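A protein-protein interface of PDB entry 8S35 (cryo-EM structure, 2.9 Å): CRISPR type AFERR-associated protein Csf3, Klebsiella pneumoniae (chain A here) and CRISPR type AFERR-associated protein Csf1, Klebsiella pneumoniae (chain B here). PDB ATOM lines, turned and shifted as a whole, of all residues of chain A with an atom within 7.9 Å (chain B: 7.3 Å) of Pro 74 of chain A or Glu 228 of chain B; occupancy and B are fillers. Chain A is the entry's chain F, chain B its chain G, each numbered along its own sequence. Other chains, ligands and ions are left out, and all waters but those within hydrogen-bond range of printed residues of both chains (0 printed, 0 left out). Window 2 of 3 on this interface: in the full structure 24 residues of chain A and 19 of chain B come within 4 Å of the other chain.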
ATOM      1  N   GLY A  71      24.113  24.528  30.853  1.00  0.00           N
ATOM      2  CA  GLY A  71      23.501  25.674  31.484  1.00  0.00           C
ATOM      3  C   GLY A  71      22.500  26.305  30.544  1.00  0.00           C
ATOM      4  O   GLY A  71      22.879  26.852  29.502  1.00  0.00           O
ATOM      5  N   ILE A  72      21.221  26.228  30.901  1.00  0.00           N
ATOM      6  CA  ILE A  72      20.134  26.779  30.102  1.00  0.00           C
ATOM      7  C   ILE A  72      19.547  27.963  30.853  1.00  0.00           C
ATOM      8  O   ILE A  72      19.283  27.874  32.057  1.00  0.00           O
ATOM      9  CB  ILE A  72      19.051  25.727  29.803  1.00  0.00           C
ATOM     10  CG1 ILE A  72      18.710  24.914  31.054  1.00  0.00           C
ATOM     11  CG2 ILE A  72      19.517  24.805  28.692  1.00  0.00           C
ATOM     12  CD1 ILE A  72      17.371  24.225  30.987  1.00  0.00           C
ATOM     13  N   THR A  73      19.353  29.060  30.150  1.00  0.00           N
ATOM     14  CA  THR A  73      18.761  30.268  30.694  1.00  0.00           C
ATOM     15  C   THR A  73      17.293  30.334  30.319  1.00  0.00           C
ATOM     16  O   THR A  73      16.832  29.612  29.432  1.00  0.00           O
ATOM     17  CB  THR A  73      19.500  31.495  30.162  1.00  0.00           C
ATOM     18  OG1 THR A  73      18.983  31.841  28.871  1.00  0.00           O
ATOM     19  CG2 THR A  73      20.987  31.222  30.050  1.00  0.00           C
ATOM     20  N   PRO A  74      16.509  31.197  30.972  1.00  0.00           N
ATOM     21  CA  PRO A  74      15.105  31.349  30.560  1.00  0.00           C
ATOM     22  C   PRO A  74      14.933  31.879  29.146  1.00  0.00           C
ATOM     23  O   PRO A  74      13.808  31.843  28.632  1.00  0.00           O
ATOM     24  CB  PRO A  74      14.530  32.327  31.595  1.00  0.00           C
ATOM     25  CG  PRO A  74      15.703  32.959  32.245  1.00  0.00           C
ATOM     26  CD  PRO A  74      16.796  31.950  32.203  1.00  0.00           C
ATOM     27  N   GLU A  75      15.995  32.363  28.501  1.00  0.00           N
ATOM     28  CA  GLU A  75      15.902  32.853  27.130  1.00  0.00           C
ATOM     29  C   GLU A  75      16.046  31.703  26.138  1.00  0.00           C
ATOM     30  O   GLU A  75      15.176  31.491  25.288  1.00  0.00           O
ATOM     31  CB  GLU A  75      16.979  33.912  26.845  1.00  0.00           C
ATOM     32  CG  GLU A  75      17.000  35.151  27.747  1.00  0.00           C
ATOM     33  CD  GLU A  75      17.482  34.864  29.156  1.00  0.00           C
ATOM     34  OE1 GLU A  75      17.714  33.680  29.470  1.00  0.00           O
ATOM     35  OE2 GLU A  75      17.659  35.818  29.938  1.00  0.00           O
ATOM     36  N   GLN A  76      17.141  30.954  26.246  1.00  0.00           N
ATOM     37  CA  GLN A  76      17.431  29.817  25.385  1.00  0.00           C
ATOM     38  C   GLN A  76      17.538  28.555  26.226  1.00  0.00           C
ATOM     39  O   GLN A  76      18.085  28.583  27.333  1.00  0.00           O
ATOM     40  CB  GLN A  76      18.730  30.037  24.607  1.00  0.00           C
ATOM     41  CG  GLN A  76      19.039  28.952  23.591  1.00  0.00           C
ATOM     42  CD  GLN A  76      20.288  29.249  22.789  1.00  0.00           C
ATOM     43  OE1 GLN A  76      20.684  30.405  22.643  1.00  0.00           O
ATOM     44  NE2 GLN A  76      20.918  28.204  22.267  1.00  0.00           N
ATOM     45  N   GLY A  77      17.016  27.450  25.694  1.00  0.00           N
ATOM     46  CA  GLY A  77      17.087  26.161  26.340  1.00  0.00           C
ATOM     47  C   GLY A  77      17.886  25.166  25.517  1.00  0.00           C
ATOM     48  O   GLY A  77      18.409  25.480  24.445  1.00  0.00           O
ATOM     49  N   PRO A 131      22.570  27.384  25.651  1.00  0.00           N
ATOM     50  CA  PRO A 131      23.276  28.669  25.669  1.00  0.00           C
ATOM     51  C   PRO A 131      24.573  28.634  26.450  1.00  0.00           C
ATOM     52  O   PRO A 131      25.442  29.478  26.198  1.00  0.00           O
ATOM     53  CB  PRO A 131      22.263  29.622  26.311  1.00  0.00           C
ATOM     54  CG  PRO A 131      21.410  28.754  27.146  1.00  0.00           C
ATOM     55  CD  PRO A 131      21.334  27.427  26.451  1.00  0.00           C
ATOM     56  N   TYR A 132      24.738  27.704  27.391  1.00  0.00           N
ATOM     57  CA  TYR A 132      25.968  27.613  28.164  1.00  0.00           C
ATOM     58  C   TYR A 132      26.313  26.159  28.433  1.00  0.00           C
ATOM     59  O   TYR A 132      25.449  25.282  28.445  1.00  0.00           O
ATOM     60  CB  TYR A 132      25.854  28.366  29.494  1.00  0.00           C
ATOM     61  CG  TYR A 132      25.615  29.840  29.317  1.00  0.00           C
ATOM     62  CD1 TYR A 132      24.331  30.339  29.186  1.00  0.00           C
ATOM     63  CD2 TYR A 132      26.673  30.731  29.268  1.00  0.00           C
ATOM     64  CE1 TYR A 132      24.107  31.679  29.013  1.00  0.00           C
ATOM     65  CE2 TYR A 132      26.455  32.078  29.098  1.00  0.00           C
ATOM     66  CZ  TYR A 132      25.168  32.544  28.968  1.00  0.00           C
ATOM     67  OH  TYR A 132      24.934  33.884  28.801  1.00  0.00           O
ATOM     68  N   LEU A 228      19.492  25.246  35.320  1.00  0.00           N
ATOM     69  CA  LEU A 228      19.304  26.679  35.159  1.00  0.00           C
ATOM     70  C   LEU A 228      20.613  27.404  35.431  1.00  0.00           C
ATOM     71  O   LEU A 228      21.349  27.061  36.361  1.00  0.00           O
ATOM     72  CB  LEU A 228      18.211  27.185  36.097  1.00  0.00           C
ATOM     73  CG  LEU A 228      16.782  27.057  35.569  1.00  0.00           C
ATOM     74  CD1 LEU A 228      15.781  27.253  36.694  1.00  0.00           C
ATOM     75  CD2 LEU A 228      16.523  28.052  34.446  1.00  0.00           C
ATOM     76  N   ILE A 229      20.907  28.413  34.611  1.00  0.00           N
ATOM     77  CA  ILE A 229      22.152  29.151  34.782  1.00  0.00           C
ATOM     78  C   ILE A 229      22.170  29.855  36.132  1.00  0.00           C
ATOM     79  O   ILE A 229      23.222  29.977  36.772  1.00  0.00           O
ATOM     80  CB  ILE A 229      22.354  30.143  33.622  1.00  0.00           C
ATOM     81  CG1 ILE A 229      23.752  30.758  33.691  1.00  0.00           C
ATOM     82  CG2 ILE A 229      21.292  31.241  33.646  1.00  0.00           C
ATOM     83  CD1 ILE A 229      24.225  31.327  32.378  1.00  0.00           C
ATOM     84  N   SER A 230      21.010  30.334  36.585  1.00  0.00           N
ATOM     85  CA  SER A 230      20.940  30.960  37.899  1.00  0.00           C
ATOM     86  C   SER A 230      21.325  29.973  38.991  1.00  0.00           C
ATOM     87  O   SER A 230      22.069  30.316  39.917  1.00  0.00           O
ATOM     88  CB  SER A 230      19.537  31.508  38.145  1.00  0.00           C
ATOM     89  OG  SER A 230      18.583  30.462  38.163  1.00  0.00           O
ATOM     90  N   LEU B 220      10.471  23.636  22.050  1.00  0.00           N
ATOM     91  CA  LEU B 220      11.565  23.787  23.001  1.00  0.00           C
ATOM     92  C   LEU B 220      12.770  22.955  22.583  1.00  0.00           C
ATOM     93  O   LEU B 220      13.909  23.434  22.620  1.00  0.00           O
ATOM     94  CB  LEU B 220      11.094  23.391  24.399  1.00  0.00           C
ATOM     95  CG  LEU B 220      12.032  23.688  25.570  1.00  0.00           C
ATOM     96  CD1 LEU B 220      12.293  25.183  25.711  1.00  0.00           C
ATOM     97  CD2 LEU B 220      11.446  23.115  26.851  1.00  0.00           C
ATOM     98  N   ILE B 225      10.937  28.241  21.023  1.00  0.00           N
ATOM     99  CA  ILE B 225      10.299  29.002  22.089  1.00  0.00           C
ATOM    100  C   ILE B 225      11.251  29.041  23.273  1.00  0.00           C
ATOM    101  O   ILE B 225      11.975  28.072  23.532  1.00  0.00           O
ATOM    102  CB  ILE B 225       8.939  28.401  22.501  1.00  0.00           C
ATOM    103  CG1 ILE B 225       9.094  26.934  22.920  1.00  0.00           C
ATOM    104  CG2 ILE B 225       7.942  28.541  21.361  1.00  0.00           C
ATOM    105  CD1 ILE B 225       7.814  26.306  23.410  1.00  0.00           C
ATOM    106  N   THR B 226      11.252  30.158  23.990  1.00  0.00           N
ATOM    107  CA  THR B 226      12.134  30.293  25.133  1.00  0.00           C
ATOM    108  C   THR B 226      11.710  29.324  26.237  1.00  0.00           C
ATOM    109  O   THR B 226      10.532  28.973  26.341  1.00  0.00           O
ATOM    110  CB  THR B 226      12.106  31.722  25.663  1.00  0.00           C
ATOM    111  OG1 THR B 226      10.805  32.011  26.186  1.00  0.00           O
ATOM    112  CG2 THR B 226      12.437  32.712  24.556  1.00  0.00           C
ATOM    113  N   PRO B 227      12.651  28.861  27.070  1.00  0.00           N
ATOM    114  CA  PRO B 227      12.255  27.982  28.180  1.00  0.00           C
ATOM    115  C   PRO B 227      11.226  28.595  29.106  1.00  0.00           C
ATOM    116  O   PRO B 227      10.392  27.865  29.653  1.00  0.00           O
ATOM    117  CB  PRO B 227      13.582  27.726  28.904  1.00  0.00           C
ATOM    118  CG  PRO B 227      14.579  27.822  27.841  1.00  0.00           C
ATOM    119  CD  PRO B 227      14.117  28.949  26.969  1.00  0.00           C
ATOM    120  N   GLU B 228      11.257  29.912  29.308  1.00  0.00           N
ATOM    121  CA  GLU B 228      10.249  30.536  30.157  1.00  0.00           C
ATOM    122  C   GLU B 228       8.864  30.403  29.539  1.00  0.00           C
ATOM    123  O   GLU B 228       7.882  30.152  30.244  1.00  0.00           O
ATOM    124  CB  GLU B 228      10.598  32.005  30.405  1.00  0.00           C
ATOM    125  CG  GLU B 228      10.688  32.866  29.154  1.00  0.00           C
ATOM    126  CD  GLU B 228      11.035  34.307  29.469  1.00  0.00           C
ATOM    127  OE1 GLU B 228      11.148  34.644  30.666  1.00  0.00           O
ATOM    128  OE2 GLU B 228      11.194  35.102  28.520  1.00  0.00           O
ATOM    129  N   ALA B 229       8.771  30.544  28.215  1.00  0.00           N
ATOM    130  CA  ALA B 229       7.482  30.391  27.550  1.00  0.00           C
ATOM    131  C   ALA B 229       6.965  28.965  27.683  1.00  0.00           C
ATOM    132  O   ALA B 229       5.783  28.750  27.975  1.00  0.00           O
ATOM    133  CB  ALA B 229       7.604  30.782  26.077  1.00  0.00           C
ATOM    134  N   ALA B 230       7.835  27.978  27.466  1.00  0.00           N
ATOM    135  CA  ALA B 230       7.418  26.589  27.608  1.00  0.00           C
ATOM    136  C   ALA B 230       6.999  26.286  29.039  1.00  0.00           C
ATOM    137  O   ALA B 230       6.016  25.573  29.269  1.00  0.00           O
ATOM    138  CB  ALA B 230       8.545  25.656  27.172  1.00  0.00           C
ATOM    139  N   SER B 231       7.742  26.807  30.017  1.00  0.00           N
ATOM    140  CA  SER B 231       7.378  26.592  31.412  1.00  0.00           C
ATOM    141  C   SER B 231       6.027  27.217  31.724  1.00  0.00           C
ATOM    142  O   SER B 231       5.211  26.626  32.441  1.00  0.00           O
ATOM    143  CB  SER B 231       8.458  27.164  32.327  1.00  0.00           C
ATOM    144  OG  SER B 231       8.544  28.572  32.190  1.00  0.00           O
ATOM    145  N   ASN B 232       5.774  28.418  31.200  1.00  0.00           N
ATOM    146  CA  ASN B 232       4.471  29.044  31.386  1.00  0.00           C
ATOM    147  C   ASN B 232       3.369  28.194  30.774  1.00  0.00           C
ATOM    148  O   ASN B 232       2.305  28.015  31.377  1.00  0.00           O
ATOM    149  CB  ASN B 232       4.469  30.442  30.772  1.00  0.00           C
ATOM    150  CG  ASN B 232       5.424  31.384  31.471  1.00  0.00           C
ATOM    151  OD1 ASN B 232       5.988  31.054  32.514  1.00  0.00           O
ATOM    152  ND2 ASN B 232       5.612  32.567  30.899  1.00  0.00           N
ATOM    153  N   GLU B 233       3.607  27.663  29.574  1.00  0.00           N
ATOM    154  CA  GLU B 233       2.598  26.831  28.927  1.00  0.00           C
ATOM    155  C   GLU B 233       2.318  25.574  29.739  1.00  0.00           C
ATOM    156  O   GLU B 233       1.159  25.181  29.911  1.00  0.00           O
ATOM    157  CB  GLU B 233       3.052  26.463  27.515  1.00  0.00           C
ATOM    158  CG  GLU B 233       3.071  27.633  26.544  1.00  0.00           C
ATOM    159  CD  GLU B 233       1.682  28.111  26.170  1.00  0.00           C
ATOM    160  OE1 GLU B 233       0.709  27.364  26.400  1.00  0.00           O
ATOM    161  OE2 GLU B 233       1.564  29.238  25.644  1.00  0.00           O
ATOM    162  N   PHE B 234       3.369  24.931  30.252  1.00  0.00           N
ATOM    163  CA  PHE B 234       3.174  23.726  31.050  1.00  0.00           C
ATOM    164  C   PHE B 234       2.429  24.034  32.340  1.00  0.00           C
ATOM    165  O   PHE B 234       1.504  23.305  32.718  1.00  0.00           O
ATOM    166  CB  PHE B 234       4.521  23.069  31.360  1.00  0.00           C
ATOM    167  CG  PHE B 234       5.289  22.629  30.141  1.00  0.00           C
ATOM    168  CD1 PHE B 234       4.647  22.047  29.061  1.00  0.00           C
ATOM    169  CD2 PHE B 234       6.663  22.784  30.088  1.00  0.00           C
ATOM    170  CE1 PHE B 234       5.357  21.643  27.950  1.00  0.00           C
ATOM    171  CE2 PHE B 234       7.377  22.382  28.977  1.00  0.00           C
ATOM    172  CZ  PHE B 234       6.724  21.811  27.909  1.00  0.00           C
ATOM    173  N   LYS B 235       2.815  25.108  33.032  1.00  0.00           N
ATOM    174  CA  LYS B 235       2.166  25.447  34.292  1.00  0.00           C
ATOM    175  C   LYS B 235       0.704  25.811  34.076  1.00  0.00           C
ATOM    176  O   LYS B 235      -0.169  25.388  34.843  1.00  0.00           O
ATOM    177  CB  LYS B 235       2.912  26.595  34.968  1.00  0.00           C
ATOM    178  CG  LYS B 235       4.253  26.191  35.553  1.00  0.00           C
ATOM    179  CD  LYS B 235       4.921  27.347  36.277  1.00  0.00           C
ATOM    180  CE  LYS B 235       5.522  28.346  35.300  1.00  0.00           C
ATOM    181  NZ  LYS B 235       6.362  29.363  35.992  1.00  0.00           N
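Among the printed residues, pairs that only touch across the chains: Thr 73 of chain A with Pro 227 of chain B (3.3 Å), Pro 74 of chain A with Thr 226 of chain B (3.4 Å), Pro 74 of chain A with Pro 227 of chain B (3.4 Å), Glu 75 of chain A with Thr 226 of chain B (3.1 Å), Glu 75 of chain A with Pro 227 of chain B (3.2 Å), Gln 76 of chain A with Pro 227 of chain B (3.4 Å) and Gly 77 of chain A with Pro 227 of chain B (3.3 Å).
O of Glu 228 of chain B lies close to OD1 of Asn 232 of chain B.
The backbone carbonyl oxygen (O) of Glu 228 of chain B lies within hydrogen-bond range of the side-chain hydroxyl (OG) of Ser 231 of chain B (2.6 Å).
The side-chain hydroxyl (OG) of Ser 231 of chain B lies within hydrogen-bond range of the backbone carbonyl oxygen (O) of Pro 227 of chain B (3.2 Å).
The side-chain hydroxyl (OG1) of Thr 73 of chain A lies within hydrogen-bond range of the backbone NH (N) of Gln 76 of chain A (3.3 Å).
The side-chain hydroxyl (OG1) of Thr 73 of chain A lies close to the backbone NH (N) of Glu 75 of chain A.
The side-chain hydroxyl (OG1) of Thr 226 of chain B lies within hydrogen-bond range of the backbone NH (N) of Ala 229 of chain B (3.2 Å).
Of the 12 printed residues of chain B, 3 touch a printed residue of chain A.
Hydrophobic or aromatic side chains of chain B that line the printed part of chain A: Pro 227.
Of the 12 printed residues of chain A, 5 touch a printed residue of chain B.
The backbone carbonyl oxygen (O) of Pro 74 of chain A lies within hydrogen-bond range of the backbone NH (N) of Glu 228 of chain B, at 3.3 Å.
Of the printed residues of chain B, Thr 73 of chain A touches Pro 227.
Of chain B, only Thr 226, Pro 227 and Glu 228 come within 4 Å of Pro 74 of chain A.
Of the printed residues of chain B, Gln 76 of chain A touches Pro 227 (3.4 Å).
Of the printed residues of chain A, Glu 228 of chain B touches Pro 74 (3.3 Å).
No residue of chain A comes within 4 Å of Ala 229 of chain B.
The nearest residue of chain B that does not touch Pro 74 of chain A is Ala 229 of chain B (5.2 Å).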
